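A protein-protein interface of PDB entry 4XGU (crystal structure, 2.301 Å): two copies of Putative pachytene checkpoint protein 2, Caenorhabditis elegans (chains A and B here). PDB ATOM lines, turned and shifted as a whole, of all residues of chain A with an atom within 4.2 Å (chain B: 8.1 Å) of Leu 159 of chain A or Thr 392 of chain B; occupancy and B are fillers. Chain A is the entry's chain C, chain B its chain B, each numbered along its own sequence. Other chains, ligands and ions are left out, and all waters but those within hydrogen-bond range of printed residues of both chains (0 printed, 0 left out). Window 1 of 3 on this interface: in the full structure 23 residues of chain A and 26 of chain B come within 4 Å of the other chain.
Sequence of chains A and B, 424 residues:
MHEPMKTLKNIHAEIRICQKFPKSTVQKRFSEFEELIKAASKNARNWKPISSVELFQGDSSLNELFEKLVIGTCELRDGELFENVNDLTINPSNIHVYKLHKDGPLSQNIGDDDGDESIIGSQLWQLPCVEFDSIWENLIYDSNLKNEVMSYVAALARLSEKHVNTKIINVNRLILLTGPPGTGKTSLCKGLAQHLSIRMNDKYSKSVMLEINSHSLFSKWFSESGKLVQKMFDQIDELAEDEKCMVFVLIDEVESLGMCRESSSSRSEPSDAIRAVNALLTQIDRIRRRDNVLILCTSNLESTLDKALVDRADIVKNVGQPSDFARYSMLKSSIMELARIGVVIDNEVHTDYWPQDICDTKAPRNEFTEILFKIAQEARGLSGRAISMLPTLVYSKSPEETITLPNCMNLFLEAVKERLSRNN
The side-chain hydroxyl (OH) of Tyr 395 of chain B sits at hydrogen-bond distance from the guanidinium group (NE) of Arg 158 of chain A (3.5 Å).
NH2 of Arg 340 of chain B lies within hydrogen-bond range of O of His 163 of chain A, 3.5 Å away.
O of Leu 393 of chain B lies within hydrogen-bond range of OG of Ser 396 of chain B.
The backbone carbonyl oxygen (O) of Tyr 395 of chain B lies within hydrogen-bond range of the side-chain hydroxyl (OG) of Ser 398 of chain B (3.0 Å).
O of Leu 156 of chain A lies within hydrogen-bond range of OG of Ser 160 of chain A (2.7 Å).
The backbone carbonyl oxygen (O) of Leu 159 of chain A sits close to the backbone NH (N) of Val 164 of chain A, 3.3 Å away.
The backbone carbonyl oxygen (O) of Leu 338 of chain B is in hydrogen-bond range of the backbone NH (N) of Val 343 of chain B, at 2.8 Å.
O of Glu 161 of chain A lies close to NE2 of His 163 of chain A (3.3 Å).
OH of Tyr 152 of chain A touches CG2 of Thr 392 of chain B (3.2 Å).
CD1 of Leu 393 of chain B touches CE2 of Tyr 152 of chain A, at 3.9 Å.
CB of Ala 155 of chain A touches O of Thr 392 of chain B, 3.6 Å away.
Tyr 395 of chain B touches Ala 155 of chain A (CD2 to O, 3.6 Å).
Ala 155 of chain A touches Ser 396 of chain B (CB to N, 3.8 Å).
Leu 156 of chain A touches Thr 392 of chain B.
Leu 338 of chain B touches Leu 159 of chain A (CD2 to CD2, 3.9 Å).
Ile 341 of chain B touches Leu 159 of chain A.
Thr 392 of chain B touches Leu 159 of chain A (CB to CD1, 3.7 Å).
Lys 162 of chain A touches Val 343 of chain B (CD to CG2, 3.9 Å).
Printed residues of chain B within 4 Å of Leu 159 of chain A: Leu 338 (3.9 Å), Ile 341 (3.98 Å), Thr 392 (3.7 Å) and Tyr 395 (3.6 Å).
Of the printed residues of chain A, Thr 392 of chain B touches Tyr 152 (3.2 Å), Ala 155 (3.6 Å), Leu 156 (3.4 Å) and Leu 159 (3.7 Å).
Of the printed residues of chain B, Tyr 152 of chain A touches Thr 392, Leu 393 and Ser 396.
Printed residues of chain A within 4 Å of Ile 341 of chain B: Leu 159 (3.98 Å), Lys 162 (3.2 Å) and Val 164 (3.7 Å).
Printed residues of chain A within 4 Å of Val 343 of chain B: Lys 162 (3.9 Å).
Ile 387 of chain B touches none of the printed residues of chain A.
Ala 415 of chain B touches none of the printed residues of chain A.
The nearest printed residue of chain A that does not touch Thr 392 of chain B is Ala 157 of chain A (6.6 Å).
Of the 11 printed residues of chain A, 8 touch a printed residue of chain B.
Of the 22 printed residues of chain B, 9 touch a printed residue of chain A.
Hydrophobic or aromatic side chains of chain B within 4 Å of the printed part of chain A: Leu 338, Ile 341, Val 343, Leu 393 and Tyr 395.
No position is printed for both chains.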
ATOM      1  N   TYR A 152     -25.159  30.032   5.477  1.00  0.00           N
ATOM      2  CA  TYR A 152     -23.796  29.710   5.875  1.00  0.00           C
ATOM      3  C   TYR A 152     -23.004  30.958   6.247  1.00  0.00           C
ATOM      4  O   TYR A 152     -22.297  30.978   7.255  1.00  0.00           O
ATOM      5  CB  TYR A 152     -23.078  28.950   4.759  1.00  0.00           C
ATOM      6  CG  TYR A 152     -21.821  28.257   5.224  1.00  0.00           C
ATOM      7  CD1 TYR A 152     -20.623  28.951   5.336  1.00  0.00           C
ATOM      8  CD2 TYR A 152     -21.833  26.912   5.560  1.00  0.00           C
ATOM      9  CE1 TYR A 152     -19.471  28.323   5.767  1.00  0.00           C
ATOM     10  CE2 TYR A 152     -20.685  26.275   5.991  1.00  0.00           C
ATOM     11  CZ  TYR A 152     -19.506  26.985   6.092  1.00  0.00           C
ATOM     12  OH  TYR A 152     -18.360  26.352   6.519  1.00  0.00           O
ATOM     13  N   ALA A 155     -24.150  32.301   9.534  1.00  0.00           N
ATOM     14  CA  ALA A 155     -23.561  31.527  10.619  1.00  0.00           C
ATOM     15  C   ALA A 155     -22.142  32.004  10.922  1.00  0.00           C
ATOM     16  O   ALA A 155     -21.751  32.105  12.083  1.00  0.00           O
ATOM     17  CB  ALA A 155     -23.564  30.046  10.278  1.00  0.00           C
ATOM     18  N   LEU A 156     -21.374  32.303   9.879  1.00  0.00           N
ATOM     19  CA  LEU A 156     -20.024  32.834  10.060  1.00  0.00           C
ATOM     20  C   LEU A 156     -20.072  34.217  10.691  1.00  0.00           C
ATOM     21  O   LEU A 156     -19.218  34.568  11.500  1.00  0.00           O
ATOM     22  CB  LEU A 156     -19.276  32.905   8.727  1.00  0.00           C
ATOM     23  CG  LEU A 156     -18.783  31.604   8.094  1.00  0.00           C
ATOM     24  CD1 LEU A 156     -18.303  31.873   6.677  1.00  0.00           C
ATOM     25  CD2 LEU A 156     -17.673  30.974   8.929  1.00  0.00           C
ATOM     26  N   ALA A 157     -21.076  34.999  10.310  1.00  0.00           N
ATOM     27  CA  ALA A 157     -21.225  36.355  10.820  1.00  0.00           C
ATOM     28  C   ALA A 157     -21.589  36.337  12.299  1.00  0.00           C
ATOM     29  O   ALA A 157     -21.021  37.087  13.089  1.00  0.00           O
ATOM     30  CB  ALA A 157     -22.274  37.113  10.021  1.00  0.00           C
ATOM     31  N   ARG A 158     -22.534  35.475  12.665  1.00  0.00           N
ATOM     32  CA  ARG A 158     -22.965  35.350  14.055  1.00  0.00           C
ATOM     33  C   ARG A 158     -21.848  34.803  14.942  1.00  0.00           C
ATOM     34  O   ARG A 158     -21.582  35.348  16.015  1.00  0.00           O
ATOM     35  CB  ARG A 158     -24.208  34.460  14.151  1.00  0.00           C
ATOM     36  CG  ARG A 158     -25.503  35.159  13.751  1.00  0.00           C
ATOM     37  CD  ARG A 158     -26.302  34.343  12.740  1.00  0.00           C
ATOM     38  NE  ARG A 158     -26.957  33.178  13.329  1.00  0.00           N
ATOM     39  CZ  ARG A 158     -27.472  32.175  12.623  1.00  0.00           C
ATOM     40  NH1 ARG A 158     -27.396  32.187  11.297  1.00  0.00           N
ATOM     41  NH2 ARG A 158     -28.055  31.155  13.238  1.00  0.00           N
ATOM     42  N   LEU A 159     -21.196  33.734  14.491  1.00  0.00           N
ATOM     43  CA  LEU A 159     -20.071  33.151  15.222  1.00  0.00           C
ATOM     44  C   LEU A 159     -18.963  34.173  15.456  1.00  0.00           C
ATOM     45  O   LEU A 159     -18.389  34.244  16.542  1.00  0.00           O
ATOM     46  CB  LEU A 159     -19.505  31.943  14.472  1.00  0.00           C
ATOM     47  CG  LEU A 159     -20.291  30.634  14.538  1.00  0.00           C
ATOM     48  CD1 LEU A 159     -19.577  29.553  13.734  1.00  0.00           C
ATOM     49  CD2 LEU A 159     -20.493  30.196  15.985  1.00  0.00           C
ATOM     50  N   SER A 160     -18.666  34.964  14.430  1.00  0.00           N
ATOM     51  CA  SER A 160     -17.630  35.982  14.533  1.00  0.00           C
ATOM     52  C   SER A 160     -18.002  37.061  15.538  1.00  0.00           C
ATOM     53  O   SER A 160     -17.178  37.461  16.362  1.00  0.00           O
ATOM     54  CB  SER A 160     -17.364  36.616  13.170  1.00  0.00           C
ATOM     55  OG  SER A 160     -16.826  35.664  12.271  1.00  0.00           O
ATOM     56  N   GLU A 161     -19.248  37.524  15.467  1.00  0.00           N
ATOM     57  CA  GLU A 161     -19.723  38.619  16.309  1.00  0.00           C
ATOM     58  C   GLU A 161     -19.666  38.243  17.786  1.00  0.00           C
ATOM     59  O   GLU A 161     -19.481  39.101  18.649  1.00  0.00           O
ATOM     60  CB  GLU A 161     -21.149  39.014  15.917  1.00  0.00           C
ATOM     61  CG  GLU A 161     -21.416  40.503  15.974  1.00  0.00           C
ATOM     62  CD  GLU A 161     -21.463  41.035  17.388  1.00  0.00           C
ATOM     63  OE1 GLU A 161     -22.060  40.366  18.259  1.00  0.00           O
ATOM     64  OE2 GLU A 161     -20.898  42.122  17.630  1.00  0.00           O
ATOM     65  N   LYS A 162     -19.815  36.953  18.066  1.00  0.00           N
ATOM     66  CA  LYS A 162     -19.755  36.457  19.435  1.00  0.00           C
ATOM     67  C   LYS A 162     -18.319  36.161  19.850  1.00  0.00           C
ATOM     68  O   LYS A 162     -18.066  35.684  20.959  1.00  0.00           O
ATOM     69  CB  LYS A 162     -20.622  35.209  19.584  1.00  0.00           C
ATOM     70  CG  LYS A 162     -22.098  35.459  19.323  1.00  0.00           C
ATOM     71  CD  LYS A 162     -22.934  34.259  19.729  1.00  0.00           C
ATOM     72  CE  LYS A 162     -24.418  34.576  19.678  1.00  0.00           C
ATOM     73  NZ  LYS A 162     -24.869  34.836  18.284  1.00  0.00           N
ATOM     74  N   HIS A 163     -17.386  36.450  18.948  1.00  0.00           N
ATOM     75  CA  HIS A 163     -15.958  36.288  19.202  1.00  0.00           C
ATOM     76  C   HIS A 163     -15.603  34.867  19.619  1.00  0.00           C
ATOM     77  O   HIS A 163     -14.952  34.655  20.640  1.00  0.00           O
ATOM     78  CB  HIS A 163     -15.494  37.284  20.267  1.00  0.00           C
ATOM     79  CG  HIS A 163     -15.820  38.707  19.938  1.00  0.00           C
ATOM     80  ND1 HIS A 163     -14.943  39.540  19.280  1.00  0.00           N
ATOM     81  CD2 HIS A 163     -16.936  39.440  20.168  1.00  0.00           C
ATOM     82  CE1 HIS A 163     -15.500  40.727  19.122  1.00  0.00           C
ATOM     83  NE2 HIS A 163     -16.710  40.693  19.653  1.00  0.00           N
ATOM     84  N   VAL A 164     -16.038  33.899  18.819  1.00  0.00           N
ATOM     85  CA  VAL A 164     -15.712  32.499  19.062  1.00  0.00           C
ATOM     86  C   VAL A 164     -14.212  32.297  18.913  1.00  0.00           C
ATOM     87  O   VAL A 164     -13.592  32.863  18.014  1.00  0.00           O
ATOM     88  CB  VAL A 164     -16.476  31.553  18.096  1.00  0.00           C
ATOM     89  CG1 VAL A 164     -16.198  31.912  16.644  1.00  0.00           C
ATOM     90  CG2 VAL A 164     -16.118  30.096  18.363  1.00  0.00           C
ATOM     91  N   SER B 334     -15.840  21.680  20.716  1.00  0.00           N
ATOM     92  CA  SER B 334     -16.606  22.562  19.845  1.00  0.00           C
ATOM     93  C   SER B 334     -17.940  22.928  20.488  1.00  0.00           C
ATOM     94  O   SER B 334     -18.323  24.097  20.520  1.00  0.00           O
ATOM     95  CB  SER B 334     -16.840  21.908  18.481  1.00  0.00           C
ATOM     96  OG  SER B 334     -15.619  21.686  17.798  1.00  0.00           O
ATOM     97  N   GLU B 337     -17.504  25.194  23.495  1.00  0.00           N
ATOM     98  CA  GLU B 337     -17.191  26.544  23.039  1.00  0.00           C
ATOM     99  C   GLU B 337     -18.431  27.219  22.472  1.00  0.00           C
ATOM    100  O   GLU B 337     -18.623  28.424  22.632  1.00  0.00           O
ATOM    101  CB  GLU B 337     -16.075  26.514  21.990  1.00  0.00           C
ATOM    102  CG  GLU B 337     -15.836  27.838  21.271  1.00  0.00           C
ATOM    103  CD  GLU B 337     -15.250  28.917  22.169  1.00  0.00           C
ATOM    104  OE1 GLU B 337     -14.900  28.619  23.333  1.00  0.00           O
ATOM    105  OE2 GLU B 337     -15.133  30.071  21.705  1.00  0.00           O
ATOM    106  N   LEU B 338     -19.275  26.434  21.812  1.00  0.00           N
ATOM    107  CA  LEU B 338     -20.536  26.946  21.292  1.00  0.00           C
ATOM    108  C   LEU B 338     -21.469  27.357  22.425  1.00  0.00           C
ATOM    109  O   LEU B 338     -22.286  28.266  22.273  1.00  0.00           O
ATOM    110  CB  LEU B 338     -21.218  25.901  20.409  1.00  0.00           C
ATOM    111  CG  LEU B 338     -20.664  25.704  18.999  1.00  0.00           C
ATOM    112  CD1 LEU B 338     -21.367  24.539  18.323  1.00  0.00           C
ATOM    113  CD2 LEU B 338     -20.820  26.977  18.181  1.00  0.00           C
ATOM    114  N   ARG B 340     -20.323  28.465  25.353  1.00  0.00           N
ATOM    115  CA  ARG B 340     -19.703  29.627  25.976  1.00  0.00           C
ATOM    116  C   ARG B 340     -20.198  30.926  25.348  1.00  0.00           C
ATOM    117  O   ARG B 340     -20.459  31.902  26.048  1.00  0.00           O
ATOM    118  CB  ARG B 340     -18.178  29.547  25.871  1.00  0.00           C
ATOM    119  CG  ARG B 340     -17.452  30.694  26.556  1.00  0.00           C
ATOM    120  CD  ARG B 340     -15.953  30.633  26.317  1.00  0.00           C
ATOM    121  NE  ARG B 340     -15.612  30.886  24.921  1.00  0.00           N
ATOM    122  CZ  ARG B 340     -15.413  32.096  24.409  1.00  0.00           C
ATOM    123  NH1 ARG B 340     -15.524  33.172  25.180  1.00  0.00           N
ATOM    124  NH2 ARG B 340     -15.107  32.234  23.126  1.00  0.00           N
ATOM    125  N   ILE B 341     -20.324  30.937  24.026  1.00  0.00           N
ATOM    126  CA  ILE B 341     -20.779  32.131  23.321  1.00  0.00           C
ATOM    127  C   ILE B 341     -22.298  32.191  23.247  1.00  0.00           C
ATOM    128  O   ILE B 341     -22.864  33.133  22.696  1.00  0.00           O
ATOM    129  CB  ILE B 341     -20.198  32.202  21.903  1.00  0.00           C
ATOM    130  CG1 ILE B 341     -20.354  30.857  21.196  1.00  0.00           C
ATOM    131  CG2 ILE B 341     -18.733  32.598  21.951  1.00  0.00           C
ATOM    132  CD1 ILE B 341     -19.689  30.807  19.839  1.00  0.00           C
ATOM    133  N   VAL B 343     -24.355  30.070  21.752  1.00  0.00           N
ATOM    134  CA  VAL B 343     -24.941  29.484  20.551  1.00  0.00           C
ATOM    135  C   VAL B 343     -25.723  28.222  20.908  1.00  0.00           C
ATOM    136  O   VAL B 343     -26.864  28.039  20.475  1.00  0.00           O
ATOM    137  CB  VAL B 343     -23.867  29.153  19.498  1.00  0.00           C
ATOM    138  CG1 VAL B 343     -24.455  28.305  18.384  1.00  0.00           C
ATOM    139  CG2 VAL B 343     -23.265  30.434  18.940  1.00  0.00           C
ATOM    140  N   VAL B 344     -25.105  27.363  21.711  1.00  0.00           N
ATOM    141  CA  VAL B 344     -25.768  26.162  22.206  1.00  0.00           C
ATOM    142  C   VAL B 344     -26.193  26.341  23.662  1.00  0.00           C
ATOM    143  O   VAL B 344     -25.362  26.314  24.571  1.00  0.00           O
ATOM    144  CB  VAL B 344     -24.859  24.921  22.082  1.00  0.00           C
ATOM    145  CG1 VAL B 344     -25.496  23.719  22.765  1.00  0.00           C
ATOM    146  CG2 VAL B 344     -24.575  24.618  20.618  1.00  0.00           C
ATOM    147  N   ALA B 386     -11.026  19.550   9.322  1.00  0.00           N
ATOM    148  CA  ALA B 386     -12.415  19.358   8.911  1.00  0.00           C
ATOM    149  C   ALA B 386     -13.362  19.340  10.107  1.00  0.00           C
ATOM    150  O   ALA B 386     -14.485  19.840  10.025  1.00  0.00           O
ATOM    151  CB  ALA B 386     -12.554  18.070   8.105  1.00  0.00           C
ATOM    152  N   ILE B 387     -12.906  18.765  11.215  1.00  0.00           N
ATOM    153  CA  ILE B 387     -13.703  18.719  12.438  1.00  0.00           C
ATOM    154  C   ILE B 387     -13.871  20.120  13.017  1.00  0.00           C
ATOM    155  O   ILE B 387     -14.916  20.451  13.576  1.00  0.00           O
ATOM    156  CB  ILE B 387     -13.064  17.793  13.488  1.00  0.00           C
ATOM    157  CG1 ILE B 387     -13.025  16.356  12.967  1.00  0.00           C
ATOM    158  CG2 ILE B 387     -13.831  17.843  14.795  1.00  0.00           C
ATOM    159  CD1 ILE B 387     -12.275  15.405  13.870  1.00  0.00           C
ATOM    160  N   SER B 388     -12.838  20.944  12.864  1.00  0.00           N
ATOM    161  CA  SER B 388     -12.900  22.337  13.289  1.00  0.00           C
ATOM    162  C   SER B 388     -13.854  23.138  12.412  1.00  0.00           C
ATOM    163  O   SER B 388     -14.407  24.147  12.846  1.00  0.00           O
ATOM    164  CB  SER B 388     -11.510  22.972  13.259  1.00  0.00           C
ATOM    165  OG  SER B 388     -10.649  22.349  14.190  1.00  0.00           O
ATOM    166  N   MET B 389     -14.032  22.681  11.174  1.00  0.00           N
ATOM    167  CA  MET B 389     -14.916  23.339  10.217  1.00  0.00           C
ATOM    168  C   MET B 389     -16.379  22.995  10.477  1.00  0.00           C
ATOM    169  O   MET B 389     -17.272  23.758  10.127  1.00  0.00           O
ATOM    170  CB  MET B 389     -14.550  22.947   8.780  1.00  0.00           C
ATOM    171  CG  MET B 389     -13.109  23.220   8.364  1.00  0.00           C
ATOM    172  SD  MET B 389     -12.842  24.796   7.526  1.00  0.00           S
ATOM    173  CE  MET B 389     -12.704  25.908   8.918  1.00  0.00           C
ATOM    174  N   LEU B 390     -16.618  21.838  11.086  1.00  0.00           N
ATOM    175  CA  LEU B 390     -17.977  21.325  11.275  1.00  0.00           C
ATOM    176  C   LEU B 390     -18.978  22.248  11.993  1.00  0.00           C
ATOM    177  O   LEU B 390     -20.123  22.349  11.552  1.00  0.00           O
ATOM    178  CB  LEU B 390     -17.923  19.987  12.016  1.00  0.00           C
ATOM    179  CG  LEU B 390     -17.636  18.757  11.156  1.00  0.00           C
ATOM    180  CD1 LEU B 390     -17.716  17.500  12.003  1.00  0.00           C
ATOM    181  CD2 LEU B 390     -18.607  18.683   9.986  1.00  0.00           C
ATOM    182  N   PRO B 391     -18.574  22.905  13.102  1.00  0.00           N
ATOM    183  CA  PRO B 391     -19.573  23.690  13.844  1.00  0.00           C
ATOM    184  C   PRO B 391     -20.295  24.769  13.031  1.00  0.00           C
ATOM    185  O   PRO B 391     -21.502  24.931  13.201  1.00  0.00           O
ATOM    186  CB  PRO B 391     -18.743  24.337  14.955  1.00  0.00           C
ATOM    187  CG  PRO B 391     -17.639  23.383  15.182  1.00  0.00           C
ATOM    188  CD  PRO B 391     -17.286  22.869  13.819  1.00  0.00           C
ATOM    189  N   THR B 392     -19.583  25.486  12.165  1.00  0.00           N
ATOM    190  CA  THR B 392     -20.207  26.565  11.404  1.00  0.00           C
ATOM    191  C   THR B 392     -21.195  26.028  10.366  1.00  0.00           C
ATOM    192  O   THR B 392     -22.110  26.735   9.951  1.00  0.00           O
ATOM    193  CB  THR B 392     -19.160  27.452  10.700  1.00  0.00           C
ATOM    194  OG1 THR B 392     -19.826  28.512  10.002  1.00  0.00           O
ATOM    195  CG2 THR B 392     -18.343  26.647   9.711  1.00  0.00           C
ATOM    196  N   LEU B 393     -21.009  24.778   9.953  1.00  0.00           N
ATOM    197  CA  LEU B 393     -21.967  24.124   9.069  1.00  0.00           C
ATOM    198  C   LEU B 393     -23.210  23.731   9.858  1.00  0.00           C
ATOM    199  O   LEU B 393     -24.330  23.813   9.356  1.00  0.00           O
ATOM    200  CB  LEU B 393     -21.346  22.894   8.402  1.00  0.00           C
ATOM    201  CG  LEU B 393     -22.252  22.094   7.461  1.00  0.00           C
ATOM    202  CD1 LEU B 393     -22.786  22.968   6.334  1.00  0.00           C
ATOM    203  CD2 LEU B 393     -21.512  20.890   6.899  1.00  0.00           C
ATOM    204  N   VAL B 394     -23.000  23.307  11.099  1.00  0.00           N
ATOM    205  CA  VAL B 394     -24.099  22.938  11.984  1.00  0.00           C
ATOM    206  C   VAL B 394     -24.960  24.154  12.315  1.00  0.00           C
ATOM    207  O   VAL B 394     -26.187  24.063  12.385  1.00  0.00           O
ATOM    208  CB  VAL B 394     -23.576  22.303  13.289  1.00  0.00           C
ATOM    209  CG1 VAL B 394     -24.724  22.002  14.239  1.00  0.00           C
ATOM    210  CG2 VAL B 394     -22.789  21.037  12.983  1.00  0.00           C
ATOM    211  N   TYR B 395     -24.306  25.295  12.503  1.00  0.00           N
ATOM    212  CA  TYR B 395     -24.991  26.533  12.853  1.00  0.00           C
ATOM    213  C   TYR B 395     -25.939  26.995  11.750  1.00  0.00           C
ATOM    214  O   TYR B 395     -27.022  27.514  12.026  1.00  0.00           O
ATOM    215  CB  TYR B 395     -23.969  27.632  13.147  1.00  0.00           C
ATOM    216  CG  TYR B 395     -24.500  28.753  14.008  1.00  0.00           C
ATOM    217  CD1 TYR B 395     -25.704  28.622  14.685  1.00  0.00           C
ATOM    218  CD2 TYR B 395     -23.799  29.945  14.139  1.00  0.00           C
ATOM    219  CE1 TYR B 395     -26.193  29.643  15.474  1.00  0.00           C
ATOM    220  CE2 TYR B 395     -24.279  30.973  14.925  1.00  0.00           C
ATOM    221  CZ  TYR B 395     -25.476  30.816  15.590  1.00  0.00           C
ATOM    222  OH  TYR B 395     -25.962  31.839  16.375  1.00  0.00           O
ATOM    223  N   SER B 396     -25.525  26.808  10.501  1.00  0.00           N
ATOM    224  CA  SER B 396     -26.320  27.247   9.358  1.00  0.00           C
ATOM    225  C   SER B 396     -27.568  26.387   9.170  1.00  0.00           C
ATOM    226  O   SER B 396     -28.610  26.879   8.734  1.00  0.00           O
ATOM    227  CB  SER B 396     -25.476  27.227   8.083  1.00  0.00           C
ATOM    228  OG  SER B 396     -25.081  25.906   7.758  1.00  0.00           O
ATOM    229  N   LYS B 397     -27.455  25.104   9.498  1.00  0.00           N
ATOM    230  CA  LYS B 397     -28.574  24.176   9.367  1.00  0.00           C
ATOM    231  C   LYS B 397     -29.692  24.471  10.364  1.00  0.00           C
ATOM    232  O   LYS B 397     -30.874  24.324  10.044  1.00  0.00           O
ATOM    233  CB  LYS B 397     -28.098  22.733   9.545  1.00  0.00           C
ATOM    234  CG  LYS B 397     -27.228  22.213   8.419  1.00  0.00           C
ATOM    235  CD  LYS B 397     -27.158  20.696   8.450  1.00  0.00           C
ATOM    236  CE  LYS B 397     -26.516  20.146   7.187  1.00  0.00           C
ATOM    237  NZ  LYS B 397     -27.221  18.925   6.706  1.00  0.00           N
ATOM    238  N   SER B 398     -29.318  24.882  11.571  1.00  0.00           N
ATOM    239  CA  SER B 398     -30.293  25.123  12.628  1.00  0.00           C
ATOM    240  C   SER B 398     -31.197  26.303  12.305  1.00  0.00           C
ATOM    241  O   SER B 398     -30.714  27.412  12.070  1.00  0.00           O
ATOM    242  CB  SER B 398     -29.595  25.373  13.963  1.00  0.00           C
ATOM    243  OG  SER B 398     -29.078  26.690  14.019  1.00  0.00           O
ATOM    244  N   PHE B 412     -25.142  17.793  14.359  1.00  0.00           N
ATOM    245  CA  PHE B 412     -23.732  17.456  14.208  1.00  0.00           C
ATOM    246  C   PHE B 412     -23.569  16.191  13.379  1.00  0.00           C
ATOM    247  O   PHE B 412     -22.721  16.127  12.490  1.00  0.00           O
ATOM    248  CB  PHE B 412     -23.066  17.282  15.575  1.00  0.00           C
ATOM    249  CG  PHE B 412     -22.240  18.463  16.003  1.00  0.00           C
ATOM    250  CD1 PHE B 412     -20.913  18.569  15.623  1.00  0.00           C
ATOM    251  CD2 PHE B 412     -22.789  19.466  16.785  1.00  0.00           C
ATOM    252  CE1 PHE B 412     -20.149  19.654  16.014  1.00  0.00           C
ATOM    253  CE2 PHE B 412     -22.029  20.553  17.181  1.00  0.00           C
ATOM    254  CZ  PHE B 412     -20.708  20.647  16.795  1.00  0.00           C
ATOM    255  N   ALA B 415     -24.235  16.921   9.697  1.00  0.00           N
ATOM    256  CA  ALA B 415     -23.131  17.648   9.083  1.00  0.00           C
ATOM    257  C   ALA B 415     -21.971  16.710   8.766  1.00  0.00           C
ATOM    258  O   ALA B 415     -21.355  16.813   7.704  1.00  0.00           O
ATOM    259  CB  ALA B 415     -22.670  18.778   9.989  1.00  0.00           C
